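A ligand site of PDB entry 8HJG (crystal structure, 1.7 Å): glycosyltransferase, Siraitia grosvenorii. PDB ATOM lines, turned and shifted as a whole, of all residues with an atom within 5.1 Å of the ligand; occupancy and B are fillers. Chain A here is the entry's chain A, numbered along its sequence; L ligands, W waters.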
ATOM      1  N   TYR A  20      -0.700  15.987  -8.934  1.00  0.00           N
ATOM      2  CA  TYR A  20      -0.138  14.732  -8.440  1.00  0.00           C
ATOM      3  C   TYR A  20      -0.836  13.517  -9.049  1.00  0.00           C
ATOM      4  O   TYR A  20      -0.194  12.497  -9.347  1.00  0.00           O
ATOM      5  CB  TYR A  20      -0.232  14.710  -6.919  1.00  0.00           C
ATOM      6  CG  TYR A  20       0.321  13.430  -6.367  1.00  0.00           C
ATOM      7  CD1 TYR A  20       1.666  13.311  -6.118  1.00  0.00           C
ATOM      8  CD2 TYR A  20      -0.512  12.351  -6.113  1.00  0.00           C
ATOM      9  CE1 TYR A  20       2.188  12.139  -5.627  1.00  0.00           C
ATOM     10  CE2 TYR A  20      -0.004  11.182  -5.622  1.00  0.00           C
ATOM     11  CZ  TYR A  20       1.350  11.074  -5.375  1.00  0.00           C
ATOM     12  OH  TYR A  20       1.864   9.900  -4.878  1.00  0.00           O
ATOM     13  N   GLY A  21      -2.149  13.597  -9.245  1.00  0.00           N
ATOM     14  CA  GLY A  21      -2.852  12.467  -9.847  1.00  0.00           C
ATOM     15  C   GLY A  21      -2.442  12.250 -11.296  1.00  0.00           C
ATOM     16  O   GLY A  21      -2.395  11.114 -11.778  1.00  0.00           O
ATOM     17  N   SER A  24       1.002  10.700 -11.215  1.00  0.00           N
ATOM     18  CA  SER A  24       0.858   9.276 -10.832  1.00  0.00           C
ATOM     19  C   SER A  24       0.508   8.424 -12.052  1.00  0.00           C
ATOM     20  O   SER A  24       1.196   7.419 -12.295  1.00  0.00           O
ATOM     21  CB  SER A  24      -0.167   9.118  -9.747  1.00  0.00           C
ATOM     22  OG  SER A  24       0.269   9.738  -8.551  1.00  0.00           O
ATOM     23  N   LYS A  55       7.576   6.697  -5.819  1.00  0.00           N
ATOM     24  CA  LYS A  55       6.778   5.684  -6.504  1.00  0.00           C
ATOM     25  C   LYS A  55       7.520   5.029  -7.665  1.00  0.00           C
ATOM     26  O   LYS A  55       6.917   4.223  -8.376  1.00  0.00           O
ATOM     27  CB  LYS A  55       5.449   6.294  -6.990  1.00  0.00           C
ATOM     28  CG  LYS A  55       4.412   6.511  -5.876  1.00  0.00           C
ATOM     29  CD  LYS A  55       3.047   6.951  -6.440  1.00  0.00           C
ATOM     30  CE  LYS A  55       1.936   6.915  -5.380  1.00  0.00           C
ATOM     31  NZ  LYS A  55       0.623   7.428  -5.924  1.00  0.00           N
ATOM     32  N   PHE A 267     -11.460   4.253   4.769  1.00  0.00           N
ATOM     33  CA  PHE A 267     -10.498   5.294   4.463  1.00  0.00           C
ATOM     34  C   PHE A 267     -11.284   6.471   3.913  1.00  0.00           C
ATOM     35  O   PHE A 267     -12.257   6.279   3.171  1.00  0.00           O
ATOM     36  CB  PHE A 267      -9.485   4.790   3.430  1.00  0.00           C
ATOM     37  CG  PHE A 267      -8.373   5.765   3.131  1.00  0.00           C
ATOM     38  CD1 PHE A 267      -7.535   6.204   4.148  1.00  0.00           C
ATOM     39  CD2 PHE A 267      -8.164   6.230   1.841  1.00  0.00           C
ATOM     40  CE1 PHE A 267      -6.517   7.102   3.874  1.00  0.00           C
ATOM     41  CE2 PHE A 267      -7.147   7.119   1.563  1.00  0.00           C
ATOM     42  CZ  PHE A 267      -6.322   7.569   2.585  1.00  0.00           C
ATOM     43  N   SER A 269     -10.720  10.248   2.059  1.00  0.00           N
ATOM     44  CA  SER A 269      -9.727  11.124   1.449  1.00  0.00           C
ATOM     45  C   SER A 269     -10.374  11.902   0.322  1.00  0.00           C
ATOM     46  O   SER A 269     -11.209  11.372  -0.420  1.00  0.00           O
ATOM     47  CB  SER A 269      -8.537  10.335   0.899  1.00  0.00           C
ATOM     48  OG  SER A 269      -7.671  11.184   0.140  1.00  0.00           O
ATOM     49  N   PHE A 270      -9.961  13.141   0.174  1.00  0.00           N
ATOM     50  CA  PHE A 270     -10.461  13.961  -0.915  1.00  0.00           C
ATOM     51  C   PHE A 270      -9.342  14.344  -1.889  1.00  0.00           C
ATOM     52  O   PHE A 270      -9.446  15.353  -2.580  1.00  0.00           O
ATOM     53  CB  PHE A 270     -11.196  15.155  -0.317  1.00  0.00           C
ATOM     54  CG  PHE A 270     -12.404  14.721   0.453  1.00  0.00           C
ATOM     55  CD1 PHE A 270     -13.599  14.507  -0.203  1.00  0.00           C
ATOM     56  CD2 PHE A 270     -12.308  14.418   1.808  1.00  0.00           C
ATOM     57  CE1 PHE A 270     -14.697  14.046   0.497  1.00  0.00           C
ATOM     58  CE2 PHE A 270     -13.407  13.948   2.504  1.00  0.00           C
ATOM     59  CZ  PHE A 270     -14.598  13.768   1.847  1.00  0.00           C
ATOM     60  N   GLY A 271      -8.311  13.508  -1.993  1.00  0.00           N
ATOM     61  CA  GLY A 271      -7.321  13.659  -3.028  1.00  0.00           C
ATOM     62  C   GLY A 271      -6.252  14.685  -2.694  1.00  0.00           C
ATOM     63  O   GLY A 271      -6.062  15.093  -1.546  1.00  0.00           O
ATOM     64  N   SER A 272      -5.564  15.114  -3.746  1.00  0.00           N
ATOM     65  CA  SER A 272      -4.367  15.937  -3.608  1.00  0.00           C
ATOM     66  C   SER A 272      -4.613  17.411  -3.870  1.00  0.00           C
ATOM     67  O   SER A 272      -3.734  18.228  -3.581  1.00  0.00           O
ATOM     68  CB  SER A 272      -3.257  15.459  -4.556  1.00  0.00           C
ATOM     69  OG  SER A 272      -3.643  15.661  -5.925  1.00  0.00           O
ATOM     70  N   GLU A 273      -5.764  17.784  -4.418  1.00  0.00           N
ATOM     71  CA  GLU A 273      -5.948  19.157  -4.841  1.00  0.00           C
ATOM     72  C   GLU A 273      -7.332  19.664  -4.468  1.00  0.00           C
ATOM     73  O   GLU A 273      -7.962  20.396  -5.228  1.00  0.00           O
ATOM     74  CB  GLU A 273      -5.681  19.305  -6.348  1.00  0.00           C
ATOM     75  CG  GLU A 273      -6.152  18.137  -7.177  1.00  0.00           C
ATOM     76  CD  GLU A 273      -5.985  18.351  -8.680  1.00  0.00           C
ATOM     77  OE1 GLU A 273      -4.857  18.181  -9.212  1.00  0.00           O
ATOM     78  OE2 GLU A 273      -6.989  18.662  -9.329  1.00  0.00           O
ATOM     79  N   VAL A 298      -7.788  11.471   6.083  1.00  0.00           N
ATOM     80  CA  VAL A 298      -6.687  12.361   5.730  1.00  0.00           C
ATOM     81  C   VAL A 298      -7.213  13.779   5.674  1.00  0.00           C
ATOM     82  O   VAL A 298      -8.085  14.095   4.853  1.00  0.00           O
ATOM     83  CB  VAL A 298      -6.031  11.975   4.391  1.00  0.00           C
ATOM     84  CG1 VAL A 298      -4.768  12.827   4.172  1.00  0.00           C
ATOM     85  CG2 VAL A 298      -5.706  10.509   4.365  1.00  0.00           C
ATOM     86  N   GLY A 331      -2.123  15.606   6.419  1.00  0.00           N
ATOM     87  CA  GLY A 331      -1.330  15.862   5.231  1.00  0.00           C
ATOM     88  C   GLY A 331      -1.359  14.808   4.147  1.00  0.00           C
ATOM     89  O   GLY A 331      -1.744  15.097   3.003  1.00  0.00           O
ATOM     90  N   TRP A 332      -0.947  13.582   4.472  1.00  0.00           N
ATOM     91  CA  TRP A 332      -0.759  12.549   3.450  1.00  0.00           C
ATOM     92  C   TRP A 332      -0.740  11.179   4.133  1.00  0.00           C
ATOM     93  O   TRP A 332      -0.121  11.019   5.195  1.00  0.00           O
ATOM     94  CB  TRP A 332       0.553  12.771   2.681  1.00  0.00           C
ATOM     95  CG  TRP A 332       0.608  12.063   1.344  1.00  0.00           C
ATOM     96  CD1 TRP A 332       1.308  10.928   1.042  1.00  0.00           C
ATOM     97  CD2 TRP A 332      -0.058  12.460   0.138  1.00  0.00           C
ATOM     98  NE1 TRP A 332       1.124  10.600  -0.287  1.00  0.00           N
ATOM     99  CE2 TRP A 332       0.278  11.519  -0.861  1.00  0.00           C
ATOM    100  CE3 TRP A 332      -0.909  13.521  -0.187  1.00  0.00           C
ATOM    101  CZ2 TRP A 332      -0.198  11.609  -2.151  1.00  0.00           C
ATOM    102  CZ3 TRP A 332      -1.386  13.602  -1.481  1.00  0.00           C
ATOM    103  CH2 TRP A 332      -1.022  12.656  -2.451  1.00  0.00           C
ATOM    104  N   ALA A 333      -1.375  10.208   3.503  1.00  0.00           N
ATOM    105  CA  ALA A 333      -1.445   8.845   4.000  1.00  0.00           C
ATOM    106  C   ALA A 333      -1.044   7.871   2.910  1.00  0.00           C
ATOM    107  O   ALA A 333      -1.157   8.179   1.720  1.00  0.00           O
ATOM    108  CB  ALA A 333      -2.860   8.520   4.488  1.00  0.00           C
ATOM    109  N   PRO A 334      -0.608   6.659   3.295  1.00  0.00           N
ATOM    110  CA  PRO A 334      -0.327   5.616   2.295  1.00  0.00           C
ATOM    111  C   PRO A 334      -1.607   4.948   1.813  1.00  0.00           C
ATOM    112  O   PRO A 334      -1.993   3.870   2.281  1.00  0.00           O
ATOM    113  CB  PRO A 334       0.587   4.640   3.048  1.00  0.00           C
ATOM    114  CG  PRO A 334       0.255   4.857   4.475  1.00  0.00           C
ATOM    115  CD  PRO A 334      -0.194   6.271   4.652  1.00  0.00           C
ATOM    116  N   GLN A 335      -2.277   5.614   0.868  1.00  0.00           N
ATOM    117  CA  GLN A 335      -3.632   5.252   0.489  1.00  0.00           C
ATOM    118  C   GLN A 335      -3.713   3.824  -0.043  1.00  0.00           C
ATOM    119  O   GLN A 335      -4.633   3.077   0.310  1.00  0.00           O
ATOM    120  CB  GLN A 335      -4.167   6.250  -0.568  1.00  0.00           C
ATOM    121  CG  GLN A 335      -5.429   5.776  -1.289  1.00  0.00           C
ATOM    122  CD  GLN A 335      -6.147   6.899  -2.009  1.00  0.00           C
ATOM    123  OE1 GLN A 335      -6.123   8.049  -1.579  1.00  0.00           O
ATOM    124  NE2 GLN A 335      -6.783   6.571  -3.134  1.00  0.00           N
ATOM    125  N   ALA A 336      -2.748   3.421  -0.869  1.00  0.00           N
ATOM    126  CA  ALA A 336      -2.806   2.079  -1.455  1.00  0.00           C
ATOM    127  C   ALA A 336      -2.656   1.015  -0.384  1.00  0.00           C
ATOM    128  O   ALA A 336      -3.451   0.058  -0.338  1.00  0.00           O
ATOM    129  CB  ALA A 336      -1.754   1.918  -2.550  1.00  0.00           C
ATOM    130  N   HIS A 350     -13.599  11.328  -2.731  1.00  0.00           N
ATOM    131  CA  HIS A 350     -14.019  12.363  -3.683  1.00  0.00           C
ATOM    132  C   HIS A 350     -14.159  11.828  -5.104  1.00  0.00           C
ATOM    133  O   HIS A 350     -14.614  12.555  -5.977  1.00  0.00           O
ATOM    134  CB  HIS A 350     -13.032  13.544  -3.646  1.00  0.00           C
ATOM    135  CG  HIS A 350     -11.754  13.306  -4.413  1.00  0.00           C
ATOM    136  ND1 HIS A 350     -10.972  12.170  -4.247  1.00  0.00           N
ATOM    137  CD2 HIS A 350     -11.100  14.082  -5.318  1.00  0.00           C
ATOM    138  CE1 HIS A 350      -9.914  12.246  -5.035  1.00  0.00           C
ATOM    139  NE2 HIS A 350      -9.965  13.395  -5.685  1.00  0.00           N
ATOM    140  N   GLY A 352     -11.937  11.133  -7.357  1.00  0.00           N
ATOM    141  CA  GLY A 352     -10.847  11.274  -8.300  1.00  0.00           C
ATOM    142  C   GLY A 352     -10.557   9.939  -8.974  1.00  0.00           C
ATOM    143  O   GLY A 352     -10.746   8.877  -8.376  1.00  0.00           O
ATOM    144  N   TRP A 353     -10.102  10.002 -10.226  1.00  0.00           N
ATOM    145  CA  TRP A 353     -10.064   8.800 -11.072  1.00  0.00           C
ATOM    146  C   TRP A 353      -9.031   7.799 -10.591  1.00  0.00           C
ATOM    147  O   TRP A 353      -9.281   6.586 -10.620  1.00  0.00           O
ATOM    148  CB  TRP A 353      -9.834   9.180 -12.546  1.00  0.00           C
ATOM    149  CG  TRP A 353     -10.051   8.011 -13.492  1.00  0.00           C
ATOM    150  CD1 TRP A 353      -9.114   7.420 -14.287  1.00  0.00           C
ATOM    151  CD2 TRP A 353     -11.274   7.284 -13.689  1.00  0.00           C
ATOM    152  NE1 TRP A 353      -9.681   6.373 -14.988  1.00  0.00           N
ATOM    153  CE2 TRP A 353     -11.009   6.275 -14.636  1.00  0.00           C
ATOM    154  CE3 TRP A 353     -12.565   7.404 -13.169  1.00  0.00           C
ATOM    155  CZ2 TRP A 353     -11.993   5.385 -15.077  1.00  0.00           C
ATOM    156  CZ3 TRP A 353     -13.549   6.514 -13.610  1.00  0.00           C
ATOM    157  CH2 TRP A 353     -13.254   5.519 -14.550  1.00  0.00           C
ATOM    158  N   ASN A 354      -7.856   8.256 -10.151  1.00  0.00           N
ATOM    159  CA  ASN A 354      -6.889   7.288  -9.626  1.00  0.00           C
ATOM    160  C   ASN A 354      -7.425   6.599  -8.384  1.00  0.00           C
ATOM    161  O   ASN A 354      -7.214   5.391  -8.213  1.00  0.00           O
ATOM    162  CB  ASN A 354      -5.550   7.957  -9.336  1.00  0.00           C
ATOM    163  CG  ASN A 354      -4.871   8.469 -10.567  1.00  0.00           C
ATOM    164  OD1 ASN A 354      -4.442   7.687 -11.431  1.00  0.00           O
ATOM    165  ND2 ASN A 354      -4.790   9.783 -10.690  1.00  0.00           N
ATOM    166  N   SER A 355      -8.129   7.337  -7.517  1.00  0.00           N
ATOM    167  CA  SER A 355      -8.700   6.718  -6.323  1.00  0.00           C
ATOM    168  C   SER A 355      -9.787   5.732  -6.693  1.00  0.00           C
ATOM    169  O   SER A 355      -9.923   4.687  -6.049  1.00  0.00           O
ATOM    170  CB  SER A 355      -9.256   7.795  -5.369  1.00  0.00           C
ATOM    171  OG  SER A 355      -8.214   8.624  -4.884  1.00  0.00           O
ATOM    172  N   GLU A 358      -7.903   2.609  -8.166  1.00  0.00           N
ATOM    173  CA  GLU A 358      -7.298   1.896  -7.049  1.00  0.00           C
ATOM    174  C   GLU A 358      -8.346   1.127  -6.268  1.00  0.00           C
ATOM    175  O   GLU A 358      -8.180  -0.065  -5.975  1.00  0.00           O
ATOM    176  CB  GLU A 358      -6.555   2.884  -6.145  1.00  0.00           C
ATOM    177  CG  GLU A 358      -5.325   3.425  -6.814  1.00  0.00           C
ATOM    178  CD  GLU A 358      -4.807   4.736  -6.221  1.00  0.00           C
ATOM    179  OE1 GLU A 358      -5.361   5.208  -5.197  1.00  0.00           O
ATOM    180  OE2 GLU A 358      -3.866   5.294  -6.820  1.00  0.00           O
ATOM    181  N   GLN A 375     -15.197  14.483 -10.950  1.00  0.00           N
ATOM    182  CA  GLN A 375     -15.623  13.605  -9.860  1.00  0.00           C
ATOM    183  C   GLN A 375     -17.098  13.237  -9.873  1.00  0.00           C
ATOM    184  O   GLN A 375     -17.416  12.059  -9.618  1.00  0.00           O
ATOM    185  CB  GLN A 375     -15.216  14.259  -8.534  1.00  0.00           C
ATOM    186  CG  GLN A 375     -13.700  14.408  -8.439  1.00  0.00           C
ATOM    187  CD  GLN A 375     -13.231  15.558  -7.571  1.00  0.00           C
ATOM    188  OE1 GLN A 375     -13.949  16.055  -6.704  1.00  0.00           O
ATOM    189  NE2 GLN A 375     -11.996  15.994  -7.813  1.00  0.00           N
HETATM  190  N1  LIG L   1      -3.103   9.745  -2.479  1.00  0.00           N
HETATM  191  C1  LIG L   1      -2.276   9.194  -1.492  1.00  0.00           C
HETATM  192  N2  LIG L   1      -2.383   9.600  -0.229  1.00  0.00           N
HETATM  193  C2  LIG L   1      -3.285  10.521   0.117  1.00  0.00           C
HETATM  194  C3  LIG L   1      -4.126  11.070  -0.839  1.00  0.00           C
HETATM  195  C4  LIG L   1      -4.006  10.662  -2.149  1.00  0.00           C
HETATM  196  O1  LIG L   1      -1.421   8.353  -1.805  1.00  0.00           O
HETATM  197  O2  LIG L   1      -3.383  10.894   1.303  1.00  0.00           O
HETATM  198  C5  LIG L   1      -2.945   9.309  -3.862  1.00  0.00           C
HETATM  199  C6  LIG L   1      -4.067   8.402  -4.322  1.00  0.00           C
HETATM  200  O3  LIG L   1      -3.743   7.049  -4.057  1.00  0.00           O
HETATM  201  C7  LIG L   1      -4.107   8.668  -5.808  1.00  0.00           C
HETATM  202  C8  LIG L   1      -3.691  10.111  -5.919  1.00  0.00           C
HETATM  203  O4  LIG L   1      -3.004  10.438  -4.707  1.00  0.00           O
HETATM  204  O5  LIG L   1      -3.135   7.866  -6.464  1.00  0.00           O
HETATM  205  C9  LIG L   1      -4.914  10.990  -6.026  1.00  0.00           C
HETATM  206  O6  LIG L   1      -5.368  11.043  -7.363  1.00  0.00           O
HETATM  207  P1  LIG L   1      -6.918  11.127  -7.696  1.00  0.00           P
HETATM  208  O7  LIG L   1      -7.652  10.164  -6.845  1.00  0.00           O
HETATM  209  O8  LIG L   1      -7.067  10.941  -9.154  1.00  0.00           O
HETATM  210  O9  LIG L   1      -7.425  12.603  -7.275  1.00  0.00           O
HETATM  211  P2  LIG L   1      -6.650  14.016  -7.126  1.00  0.00           P
HETATM  212  O10 LIG L   1      -7.792  14.963  -7.139  1.00  0.00           O
HETATM  213  O11 LIG L   1      -5.869  13.928  -5.880  1.00  0.00           O
HETATM  214  O12 LIG L   1      -5.571  14.243  -8.086  1.00  0.00           O
HETATM  215  O   HOH W   1      -7.316  10.249  -2.421  1.00  0.00           O
HETATM  216  O   HOH W   2      -0.576   5.154  -1.954  1.00  0.00           O
HETATM  217  O   HOH W   3      -4.049  15.674  -9.565  1.00  0.00           O
HETATM  218  O   HOH W   4       1.025   7.281  -0.881  1.00  0.00           O
HETATM  219  O   HOH W   5      -8.324  16.548  -4.990  1.00  0.00           O
HETATM  220  O   HOH W   6      -1.372   5.720  -4.382  1.00  0.00           O
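The backbone NH (N) of Ser 272 lies within hydrogen-bond range of an oxygen (O11) of the ligand (2.5 Å). The side-chain hydroxyl of Ser 272 sits at hydrogen-bond distance from an oxygen (O11) of the ligand, 2.8 Å away. The backbone NH (N) of Ser 355 lies within hydrogen-bond range of an oxygen (O7) of the ligand, 2.9 Å away. The side-chain hydroxyl of Ser 355 is in hydrogen-bond range of an oxygen (O7) of the ligand (2.6 Å). O5 of the ligand lies within hydrogen-bond range of OE2 of Glu 358. The backbone NH (N) of Ala 333 sits at hydrogen-bond distance from an oxygen (O2) of the ligand, 3.1 Å away. O of Ala 333 is in hydrogen-bond range of N2 of the ligand, 2.7 Å away. An oxygen (O8) of the ligand lies within hydrogen-bond range of the backbone NH of Asn 354 (3.0 Å). O8 of the ligand lies within hydrogen-bond range of ND2 of Asn 354 (3.0 Å). A ring nitrogen (NE2) of His 350 is in hydrogen-bond range of an oxygen (O10) of the ligand (3.0 Å). NE2 of Gln 335 sits close to O3 of the ligand (3.2 Å). The backbone NH (N) of Trp 353 lies within hydrogen-bond range of an oxygen (O8) of the ligand (3.4 Å).
The side-chain hydroxyl of Ser 355 lies within hydrogen-bond range of the side-chain amide nitrogen of Gln 335, at 3.1 Å. OE1 of Glu 358 is in hydrogen-bond range of NE2 of Gln 335. The backbone carbonyl oxygen (O) of Gly 21 sits at hydrogen-bond distance from the side-chain amide nitrogen (ND2) of Asn 354. A ring nitrogen (ND1) of His 350 lies close to the backbone NH of Gly 352. The backbone carbonyl oxygen (O) of Ser 269 lies within hydrogen-bond range of the backbone NH (N) of His 350 (3.3 Å). OG of Ser 269 lies within hydrogen-bond range of N of Gly 271, at 3.2 Å. NZ of Lys 55 is in hydrogen-bond range of OH of Tyr 20 (3.0 Å). O of Tyr 20 is in hydrogen-bond range of OG of Ser 24 (2.9 Å).
Tyr 20 touches the ligand. N of Gly 21 touches O12 of the ligand, 3.7 Å away. Lys 55 touches the ligand (NZ to O5, 3.8 Å). Ser 269 touches the ligand. Gly 271 touches the ligand. Glu 273 touches the ligand (CG to O10, 3.6 Å). CG1 of Val 298 touches O2 of the ligand, 3.7 Å away. CZ2 of Trp 332 touches C1 of the ligand (3.3 Å). C of Gly 352 touches O7 of the ligand (3.6 Å). 17 residues have an atom within 4 Å of the ligand: Tyr 20, Gly 21, Lys 55, Ser 269, Gly 271, Ser 272, Glu 273, Val 298, Trp 332, Ala 333, Gln 335, His 350, Gly 352, Trp 353, Asn 354, Ser 355 and Glu 358. The nearest printed residue that does not touch the ligand is Gln 375 (4.4 Å).
Water W3 lies within hydrogen-bond range of an oxygen (O12) of the ligand (2.6 Å), the side-chain carboxylate of Glu 273 (2.7 Å), the backbone NH of Gly 21 (2.8 Å) and the backbone NH of Tyr 20 (3.4 Å). Water W5 lies within hydrogen-bond range of O10 of the ligand (2.7 Å), N of Glu 273 (2.9 Å), O of Phe 270 (2.9 Å) and N of Ser 272 (3.3 Å). Water W6 lies within hydrogen-bond range of O3 of the ligand (2.7 Å) and NZ of Lys 55 (3.0 Å). Water W4 bridges O1 of the ligand and NE1 of Trp 332. Water W2 lies within hydrogen-bond range of the backbone NH (N) of Ala 336 (3.0 Å), an oxygen (O1) of the ligand (3.3 Å) and the backbone NH (N) of Gln 335 (3.3 Å). Water W1 lies within hydrogen-bond range of OE1 of Gln 335 (2.6 Å), OG of Ser 269 (2.7 Å), OG of Ser 355 (3.1 Å) and N of Gly 271 (3.4 Å).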
